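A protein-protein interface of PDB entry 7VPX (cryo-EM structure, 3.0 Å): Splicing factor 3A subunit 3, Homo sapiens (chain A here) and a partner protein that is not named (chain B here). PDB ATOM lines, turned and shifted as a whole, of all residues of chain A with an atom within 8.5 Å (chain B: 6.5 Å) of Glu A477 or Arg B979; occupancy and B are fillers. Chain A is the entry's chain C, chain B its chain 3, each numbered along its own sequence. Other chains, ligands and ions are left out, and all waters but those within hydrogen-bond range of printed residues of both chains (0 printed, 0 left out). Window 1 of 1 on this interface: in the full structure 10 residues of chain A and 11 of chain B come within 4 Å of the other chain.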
ATOM      1  N   TRP A 471      15.365 -21.041  13.213  1.00  0.00           N
ATOM      2  CA  TRP A 471      14.400 -20.350  14.059  1.00  0.00           C
ATOM      3  C   TRP A 471      14.567 -18.848  13.860  1.00  0.00           C
ATOM      4  O   TRP A 471      15.544 -18.261  14.339  1.00  0.00           O
ATOM      5  CB  TRP A 471      14.597 -20.727  15.528  1.00  0.00           C
ATOM      6  CG  TRP A 471      14.008 -19.743  16.504  1.00  0.00           C
ATOM      7  CD1 TRP A 471      14.695 -18.944  17.372  1.00  0.00           C
ATOM      8  CD2 TRP A 471      12.621 -19.473  16.725  1.00  0.00           C
ATOM      9  NE1 TRP A 471      13.821 -18.187  18.110  1.00  0.00           N
ATOM     10  CE2 TRP A 471      12.541 -18.490  17.731  1.00  0.00           C
ATOM     11  CE3 TRP A 471      11.436 -19.958  16.164  1.00  0.00           C
ATOM     12  CZ2 TRP A 471      11.328 -17.988  18.188  1.00  0.00           C
ATOM     13  CZ3 TRP A 471      10.232 -19.459  16.622  1.00  0.00           C
ATOM     14  CH2 TRP A 471      10.187 -18.488  17.627  1.00  0.00           C
ATOM     15  N   GLN A 472      13.625 -18.233  13.154  1.00  0.00           N
ATOM     16  CA  GLN A 472      13.679 -16.799  12.888  1.00  0.00           C
ATOM     17  C   GLN A 472      12.694 -16.070  13.790  1.00  0.00           C
ATOM     18  O   GLN A 472      11.497 -16.017  13.473  1.00  0.00           O
ATOM     19  CB  GLN A 472      13.381 -16.504  11.418  1.00  0.00           C
ATOM     20  CG  GLN A 472      12.458 -17.508  10.750  1.00  0.00           C
ATOM     21  CD  GLN A 472      13.193 -18.417   9.788  1.00  0.00           C
ATOM     22  OE1 GLN A 472      14.085 -17.980   9.064  1.00  0.00           O
ATOM     23  NE2 GLN A 472      12.819 -19.691   9.774  1.00  0.00           N
ATOM     24  N   PRO A 473      13.146 -15.485  14.902  1.00  0.00           N
ATOM     25  CA  PRO A 473      12.193 -14.906  15.863  1.00  0.00           C
ATOM     26  C   PRO A 473      11.427 -13.704  15.334  1.00  0.00           C
ATOM     27  O   PRO A 473      10.321 -13.426  15.813  1.00  0.00           O
ATOM     28  CB  PRO A 473      13.088 -14.532  17.051  1.00  0.00           C
ATOM     29  CG  PRO A 473      14.440 -14.344  16.459  1.00  0.00           C
ATOM     30  CD  PRO A 473      14.543 -15.329  15.337  1.00  0.00           C
ATOM     31  N   ASP A 474      11.981 -12.979  14.358  1.00  0.00           N
ATOM     32  CA  ASP A 474      11.339 -11.754  13.886  1.00  0.00           C
ATOM     33  C   ASP A 474       9.957 -12.035  13.309  1.00  0.00           C
ATOM     34  O   ASP A 474       8.975 -11.373  13.667  1.00  0.00           O
ATOM     35  CB  ASP A 474      12.221 -11.064  12.845  1.00  0.00           C
ATOM     36  CG  ASP A 474      13.683 -11.070  13.229  1.00  0.00           C
ATOM     37  OD1 ASP A 474      14.490 -11.677  12.491  1.00  0.00           O
ATOM     38  OD2 ASP A 474      14.026 -10.468  14.267  1.00  0.00           O
ATOM     39  N   THR A 475       9.860 -13.011  12.404  1.00  0.00           N
ATOM     40  CA  THR A 475       8.573 -13.325  11.792  1.00  0.00           C
ATOM     41  C   THR A 475       7.874 -14.453  12.546  1.00  0.00           C
ATOM     42  O   THR A 475       6.642 -14.559  12.530  1.00  0.00           O
ATOM     43  CB  THR A 475       8.761 -13.686  10.317  1.00  0.00           C
ATOM     44  OG1 THR A 475       7.574 -14.319   9.822  1.00  0.00           O
ATOM     45  CG2 THR A 475       9.950 -14.621  10.128  1.00  0.00           C
ATOM     46  N   GLU A 476       8.645 -15.301  13.217  1.00  0.00           N
ATOM     47  CA  GLU A 476       8.102 -16.377  14.032  1.00  0.00           C
ATOM     48  C   GLU A 476       8.139 -15.965  15.494  1.00  0.00           C
ATOM     49  O   GLU A 476       9.161 -16.143  16.164  1.00  0.00           O
ATOM     50  CB  GLU A 476       8.891 -17.670  13.837  1.00  0.00           C
ATOM     51  CG  GLU A 476       8.317 -18.606  12.805  1.00  0.00           C
ATOM     52  CD  GLU A 476       9.233 -19.778  12.533  1.00  0.00           C
ATOM     53  OE1 GLU A 476      10.337 -19.559  11.994  1.00  0.00           O
ATOM     54  OE2 GLU A 476       8.856 -20.918  12.873  1.00  0.00           O
ATOM     55  N   GLU A 477       7.034 -15.399  15.972  1.00  0.00           N
ATOM     56  CA  GLU A 477       6.845 -15.080  17.381  1.00  0.00           C
ATOM     57  C   GLU A 477       5.420 -14.590  17.574  1.00  0.00           C
ATOM     58  O   GLU A 477       4.808 -14.060  16.642  1.00  0.00           O
ATOM     59  CB  GLU A 477       7.849 -14.028  17.860  1.00  0.00           C
ATOM     60  CG  GLU A 477       8.037 -13.994  19.365  1.00  0.00           C
ATOM     61  CD  GLU A 477       9.494 -14.079  19.765  1.00  0.00           C
ATOM     62  OE1 GLU A 477       9.811 -13.806  20.939  1.00  0.00           O
ATOM     63  OE2 GLU A 477      10.321 -14.426  18.900  1.00  0.00           O
ATOM     64  N   GLU A 478       4.882 -14.755  18.779  1.00  0.00           N
ATOM     65  CA  GLU A 478       3.507 -14.372  19.080  1.00  0.00           C
ATOM     66  C   GLU A 478       3.546 -13.380  20.236  1.00  0.00           C
ATOM     67  O   GLU A 478       3.709 -13.771  21.395  1.00  0.00           O
ATOM     68  CB  GLU A 478       2.654 -15.590  19.416  1.00  0.00           C
ATOM     69  N   TYR A 479       3.417 -12.098  19.913  1.00  0.00           N
ATOM     70  CA  TYR A 479       3.273 -11.070  20.929  1.00  0.00           C
ATOM     71  C   TYR A 479       1.830 -10.584  20.958  1.00  0.00           C
ATOM     72  O   TYR A 479       1.158 -10.552  19.924  1.00  0.00           O
ATOM     73  CB  TYR A 479       4.224  -9.905  20.656  1.00  0.00           C
ATOM     74  N   GLU A 480       1.359 -10.214  22.143  1.00  0.00           N
ATOM     75  CA  GLU A 480       0.023  -9.648  22.338  1.00  0.00           C
ATOM     76  C   GLU A 480       0.214  -8.305  23.031  1.00  0.00           C
ATOM     77  O   GLU A 480       0.417  -8.238  24.246  1.00  0.00           O
ATOM     78  CB  GLU A 480      -0.875 -10.596  23.147  1.00  0.00           C
ATOM     79  N   LYS A 489      -3.585 -11.006  19.477  1.00  0.00           N
ATOM     80  CA  LYS A 489      -2.361 -11.775  19.656  1.00  0.00           C
ATOM     81  C   LYS A 489      -1.653 -12.045  18.334  1.00  0.00           C
ATOM     82  O   LYS A 489      -0.641 -12.759  18.326  1.00  0.00           O
ATOM     83  CB  LYS A 489      -2.653 -13.103  20.369  1.00  0.00           C
ATOM     84  N   LYS A 490      -2.150 -11.504  17.220  1.00  0.00           N
ATOM     85  CA  LYS A 490      -1.519 -11.707  15.922  1.00  0.00           C
ATOM     86  C   LYS A 490      -0.395 -10.718  15.651  1.00  0.00           C
ATOM     87  O   LYS A 490       0.069 -10.635  14.507  1.00  0.00           O
ATOM     88  CB  LYS A 490      -2.565 -11.614  14.810  1.00  0.00           C
ATOM     89  N   THR A 491       0.050  -9.971  16.656  1.00  0.00           N
ATOM     90  CA  THR A 491       1.125  -9.006  16.467  1.00  0.00           C
ATOM     91  C   THR A 491       2.454  -9.729  16.280  1.00  0.00           C
ATOM     92  O   THR A 491       2.788 -10.637  17.049  1.00  0.00           O
ATOM     93  CB  THR A 491       1.196  -8.054  17.658  1.00  0.00           C
ATOM     94  N   TYR A 492       3.206  -9.331  15.260  1.00  0.00           N
ATOM     95  CA  TYR A 492       4.548  -9.851  15.041  1.00  0.00           C
ATOM     96  C   TYR A 492       5.513  -9.172  16.011  1.00  0.00           C
ATOM     97  O   TYR A 492       5.111  -8.424  16.905  1.00  0.00           O
ATOM     98  CB  TYR A 492       4.961  -9.660  13.583  1.00  0.00           C
ATOM     99  N   GLU A 493       6.811  -9.427  15.844  1.00  0.00           N
ATOM    100  CA  GLU A 493       7.801  -8.813  16.721  1.00  0.00           C
ATOM    101  C   GLU A 493       8.104  -7.373  16.335  1.00  0.00           C
ATOM    102  O   GLU A 493       8.708  -6.646  17.130  1.00  0.00           O
ATOM    103  CB  GLU A 493       9.091  -9.636  16.716  1.00  0.00           C
ATOM    104  N   ASP A 494       7.706  -6.946  15.137  1.00  0.00           N
ATOM    105  CA  ASP A 494       7.916  -5.576  14.687  1.00  0.00           C
ATOM    106  C   ASP A 494       6.734  -4.663  14.971  1.00  0.00           C
ATOM    107  O   ASP A 494       6.937  -3.505  15.349  1.00  0.00           O
ATOM    108  CB  ASP A 494       8.218  -5.551  13.185  1.00  0.00           C
ATOM    109  N   GLU B 946      -0.720 -27.629  14.557  1.00  0.00           N
ATOM    110  CA  GLU B 946      -0.755 -28.359  13.297  1.00  0.00           C
ATOM    111  C   GLU B 946      -0.376 -29.827  13.438  1.00  0.00           C
ATOM    112  O   GLU B 946      -0.175 -30.497  12.421  1.00  0.00           O
ATOM    113  CB  GLU B 946       0.172 -27.690  12.280  1.00  0.00           C
ATOM    114  CG  GLU B 946       1.604 -27.500  12.760  1.00  0.00           C
ATOM    115  CD  GLU B 946       1.817 -26.195  13.509  1.00  0.00           C
ATOM    116  OE1 GLU B 946       0.865 -25.702  14.150  1.00  0.00           O
ATOM    117  OE2 GLU B 946       2.942 -25.658  13.452  1.00  0.00           O
ATOM    118  N   ARG B 968       8.506 -26.602  21.296  1.00  0.00           N
ATOM    119  CA  ARG B 968       8.164 -25.190  21.378  1.00  0.00           C
ATOM    120  C   ARG B 968       8.063 -24.747  22.829  1.00  0.00           C
ATOM    121  O   ARG B 968       7.760 -25.535  23.730  1.00  0.00           O
ATOM    122  CB  ARG B 968       6.846 -24.895  20.650  1.00  0.00           C
ATOM    123  CG  ARG B 968       6.941 -24.962  19.140  1.00  0.00           C
ATOM    124  CD  ARG B 968       5.568 -24.907  18.515  1.00  0.00           C
ATOM    125  NE  ARG B 968       5.630 -24.782  17.064  1.00  0.00           N
ATOM    126  CZ  ARG B 968       4.575 -24.874  16.265  1.00  0.00           C
ATOM    127  NH1 ARG B 968       3.371 -25.092  16.776  1.00  0.00           N
ATOM    128  NH2 ARG B 968       4.720 -24.748  14.956  1.00  0.00           N
ATOM    129  N   VAL B 969       8.318 -23.457  23.041  1.00  0.00           N
ATOM    130  CA  VAL B 969       8.102 -22.783  24.317  1.00  0.00           C
ATOM    131  C   VAL B 969       6.835 -21.951  24.153  1.00  0.00           C
ATOM    132  O   VAL B 969       6.620 -21.349  23.095  1.00  0.00           O
ATOM    133  CB  VAL B 969       9.291 -21.903  24.723  1.00  0.00           C
ATOM    134  CG1 VAL B 969       9.001 -21.185  26.027  1.00  0.00           C
ATOM    135  CG2 VAL B 969      10.552 -22.733  24.853  1.00  0.00           C
ATOM    136  N   TYR B 970       6.001 -21.922  25.184  1.00  0.00           N
ATOM    137  CA  TYR B 970       4.707 -21.258  25.144  1.00  0.00           C
ATOM    138  C   TYR B 970       4.484 -20.472  26.432  1.00  0.00           C
ATOM    139  O   TYR B 970       4.678 -20.978  27.539  1.00  0.00           O
ATOM    140  CB  TYR B 970       3.582 -22.276  24.943  1.00  0.00           C
ATOM    141  CG  TYR B 970       3.247 -22.576  23.506  1.00  0.00           C
ATOM    142  CD1 TYR B 970       2.599 -21.642  22.715  1.00  0.00           C
ATOM    143  CD2 TYR B 970       3.569 -23.803  22.940  1.00  0.00           C
ATOM    144  CE1 TYR B 970       2.285 -21.915  21.401  1.00  0.00           C
ATOM    145  CE2 TYR B 970       3.260 -24.085  21.626  1.00  0.00           C
ATOM    146  CZ  TYR B 970       2.617 -23.137  20.862  1.00  0.00           C
ATOM    147  OH  TYR B 970       2.307 -23.415  19.554  1.00  0.00           O
ATOM    148  N   ASP B 971       4.066 -19.219  26.280  1.00  0.00           N
ATOM    149  CA  ASP B 971       3.681 -18.406  27.426  1.00  0.00           C
ATOM    150  C   ASP B 971       2.173 -18.213  27.392  1.00  0.00           C
ATOM    151  O   ASP B 971       1.543 -18.322  26.338  1.00  0.00           O
ATOM    152  CB  ASP B 971       4.409 -17.059  27.431  1.00  0.00           C
ATOM    153  CG  ASP B 971       4.387 -16.389  28.792  1.00  0.00           C
ATOM    154  OD1 ASP B 971       3.738 -16.922  29.716  1.00  0.00           O
ATOM    155  OD2 ASP B 971       5.025 -15.325  28.941  1.00  0.00           O
ATOM    156  N   LEU B 977      -2.237 -19.283  23.592  1.00  0.00           N
ATOM    157  CA  LEU B 977      -0.859 -19.453  24.026  1.00  0.00           C
ATOM    158  C   LEU B 977       0.090 -18.889  22.974  1.00  0.00           C
ATOM    159  O   LEU B 977      -0.083 -19.092  21.771  1.00  0.00           O
ATOM    160  CB  LEU B 977      -0.546 -20.928  24.286  1.00  0.00           C
ATOM    161  CG  LEU B 977      -1.344 -21.614  25.397  1.00  0.00           C
ATOM    162  CD1 LEU B 977      -1.164 -23.113  25.325  1.00  0.00           C
ATOM    163  CD2 LEU B 977      -0.927 -21.092  26.758  1.00  0.00           C
ATOM    164  N   LEU B 978       1.100 -18.171  23.451  1.00  0.00           N
ATOM    165  CA  LEU B 978       1.998 -17.399  22.595  1.00  0.00           C
ATOM    166  C   LEU B 978       3.292 -18.180  22.406  1.00  0.00           C
ATOM    167  O   LEU B 978       3.989 -18.488  23.377  1.00  0.00           O
ATOM    168  CB  LEU B 978       2.260 -16.023  23.201  1.00  0.00           C
ATOM    169  CG  LEU B 978       1.010 -15.186  23.469  1.00  0.00           C
ATOM    170  CD1 LEU B 978       1.357 -13.963  24.294  1.00  0.00           C
ATOM    171  CD2 LEU B 978       0.338 -14.786  22.169  1.00  0.00           C
ATOM    172  N   ARG B 979       3.611 -18.502  21.154  1.00  0.00           N
ATOM    173  CA  ARG B 979       4.847 -19.206  20.839  1.00  0.00           C
ATOM    174  C   ARG B 979       6.038 -18.280  21.051  1.00  0.00           C
ATOM    175  O   ARG B 979       6.031 -17.135  20.591  1.00  0.00           O
ATOM    176  CB  ARG B 979       4.808 -19.717  19.403  1.00  0.00           C
ATOM    177  CG  ARG B 979       6.061 -20.458  18.981  1.00  0.00           C
ATOM    178  CD  ARG B 979       5.789 -21.370  17.802  1.00  0.00           C
ATOM    179  NE  ARG B 979       5.998 -20.704  16.522  1.00  0.00           N
ATOM    180  CZ  ARG B 979       5.023 -20.340  15.700  1.00  0.00           C
ATOM    181  NH1 ARG B 979       3.758 -20.575  16.023  1.00  0.00           N
ATOM    182  NH2 ARG B 979       5.309 -19.742  14.552  1.00  0.00           N
ATOM    183  N   LYS B 980       7.064 -18.778  21.739  1.00  0.00           N
ATOM    184  CA  LYS B 980       8.201 -17.963  22.145  1.00  0.00           C
ATOM    185  C   LYS B 980       9.521 -18.455  21.564  1.00  0.00           C
ATOM    186  O   LYS B 980      10.375 -17.644  21.194  1.00  0.00           O
ATOM    187  CB  LYS B 980       8.289 -17.921  23.673  1.00  0.00           C
ATOM    188  CG  LYS B 980       7.239 -17.042  24.320  1.00  0.00           C
ATOM    189  CD  LYS B 980       7.485 -15.579  24.008  1.00  0.00           C
ATOM    190  CE  LYS B 980       6.392 -14.702  24.582  1.00  0.00           C
ATOM    191  NZ  LYS B 980       5.268 -14.525  23.630  1.00  0.00           N
ATOM    192  N   CYS B 981       9.712 -19.768  21.485  1.00  0.00           N
ATOM    193  CA  CYS B 981      10.929 -20.347  20.941  1.00  0.00           C
ATOM    194  C   CYS B 981      10.588 -21.682  20.297  1.00  0.00           C
ATOM    195  O   CYS B 981       9.530 -22.259  20.553  1.00  0.00           O
ATOM    196  CB  CYS B 981      12.003 -20.529  22.022  1.00  0.00           C
ATOM    197  SG  CYS B 981      13.681 -20.723  21.391  1.00  0.00           S
ATOM    198  N   GLU B 982      11.500 -22.173  19.460  1.00  0.00           N
ATOM    199  CA  GLU B 982      11.225 -23.388  18.706  1.00  0.00           C
ATOM    200  C   GLU B 982      12.526 -24.017  18.231  1.00  0.00           C
ATOM    201  O   GLU B 982      13.415 -23.314  17.743  1.00  0.00           O
ATOM    202  CB  GLU B 982      10.313 -23.087  17.515  1.00  0.00           C
ATOM    203  CG  GLU B 982      10.109 -24.253  16.576  1.00  0.00           C
ATOM    204  CD  GLU B 982       8.978 -24.018  15.597  1.00  0.00           C
ATOM    205  OE1 GLU B 982       8.502 -22.868  15.502  1.00  0.00           O
ATOM    206  OE2 GLU B 982       8.569 -24.978  14.916  1.00  0.00           O
ATOM    207  N   ASN B1019      17.344 -16.719  23.823  1.00  0.00           N
ATOM    208  CA  ASN B1019      16.066 -17.290  23.398  1.00  0.00           C
ATOM    209  C   ASN B1019      16.280 -18.349  22.311  1.00  0.00           C
ATOM    210  O   ASN B1019      15.776 -18.256  21.191  1.00  0.00           O
ATOM    211  CB  ASN B1019      15.109 -16.188  22.924  1.00  0.00           C
ATOM    212  CG  ASN B1019      13.655 -16.601  23.010  1.00  0.00           C
ATOM    213  OD1 ASN B1019      13.197 -17.097  24.038  1.00  0.00           O
ATOM    214  ND2 ASN B1019      12.922 -16.405  21.924  1.00  0.00           N
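The backbone carbonyl oxygen (O) of Arg B979 lies within hydrogen-bond range of the backbone NH (N) of Glu A478, 3.2 Å away.
NZ of Lys B980 is in hydrogen-bond range of O of Glu A478 (2.8 Å).
The side-chain carboxylate (OE2) of Glu A476 sits close to the side-chain carboxylate (OE1) of Glu B982, 3.3 Å away.
O of Val B969 lies within hydrogen-bond range of N of Lys B980, 2.9 Å away.
N of Val B969 is in hydrogen-bond range of O of Cys B981 (3.0 Å).
The backbone carbonyl oxygen of Asp B971 is in hydrogen-bond range of the backbone NH of Leu B978 (2.9 Å).
NE of Arg B979 is in salt-bridge range of OE1 of Glu B982, 3.5 Å away.
The side-chain amide nitrogen (ND2) of Asn B1019 lies within hydrogen-bond range of the backbone carbonyl oxygen (O) of Lys B980, 2.9 Å away.
The backbone carbonyl oxygen (O) of Asn B1019 lies within hydrogen-bond range of the side-chain sulfur (SG) of Cys B981.
Among the printed residues, merely in contact across the chains: Trp A471 with Lys B980 (3.2 Å), Glu A478 with Leu B978 (3.2 Å), Trp A471 with Glu B982 (3.6 Å), Trp A471 with Cys B981 (3.6 Å), Trp A471 with Asn B1019 (3.6 Å), Glu A476 with Arg B979 (3.7 Å), Lys A489 with Leu B978 (3.9 Å), Glu A477 with Lys B980 (3.9 Å) and Glu A477 with Arg B979 (3.9 Å).
Printed residues of chain B within 4 Å of Glu A476: Arg B979 and Glu B982.
Arg B979 touches just these residues of chain A: Glu A476, Glu A477 and Glu A478.
Of the printed residues of chain A, Glu B982 touches Trp A471 and Glu A476.
The nearest residue of chain B that does not touch Glu A477 is Asn B1019 (4.2 Å).
The nearest residue of chain A that does not touch Arg B979 is Trp A471 (4.4 Å).
The nearest printed residue of chain A that does not touch Lys B980 is Tyr A479 (4.8 Å).
Among the printed residues, 12 pairs touch across the chains.
Among the printed residues, no Asp or Glu carboxylate lies within 4 Å of a Lys or Arg side-chain nitrogen of the other chain.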
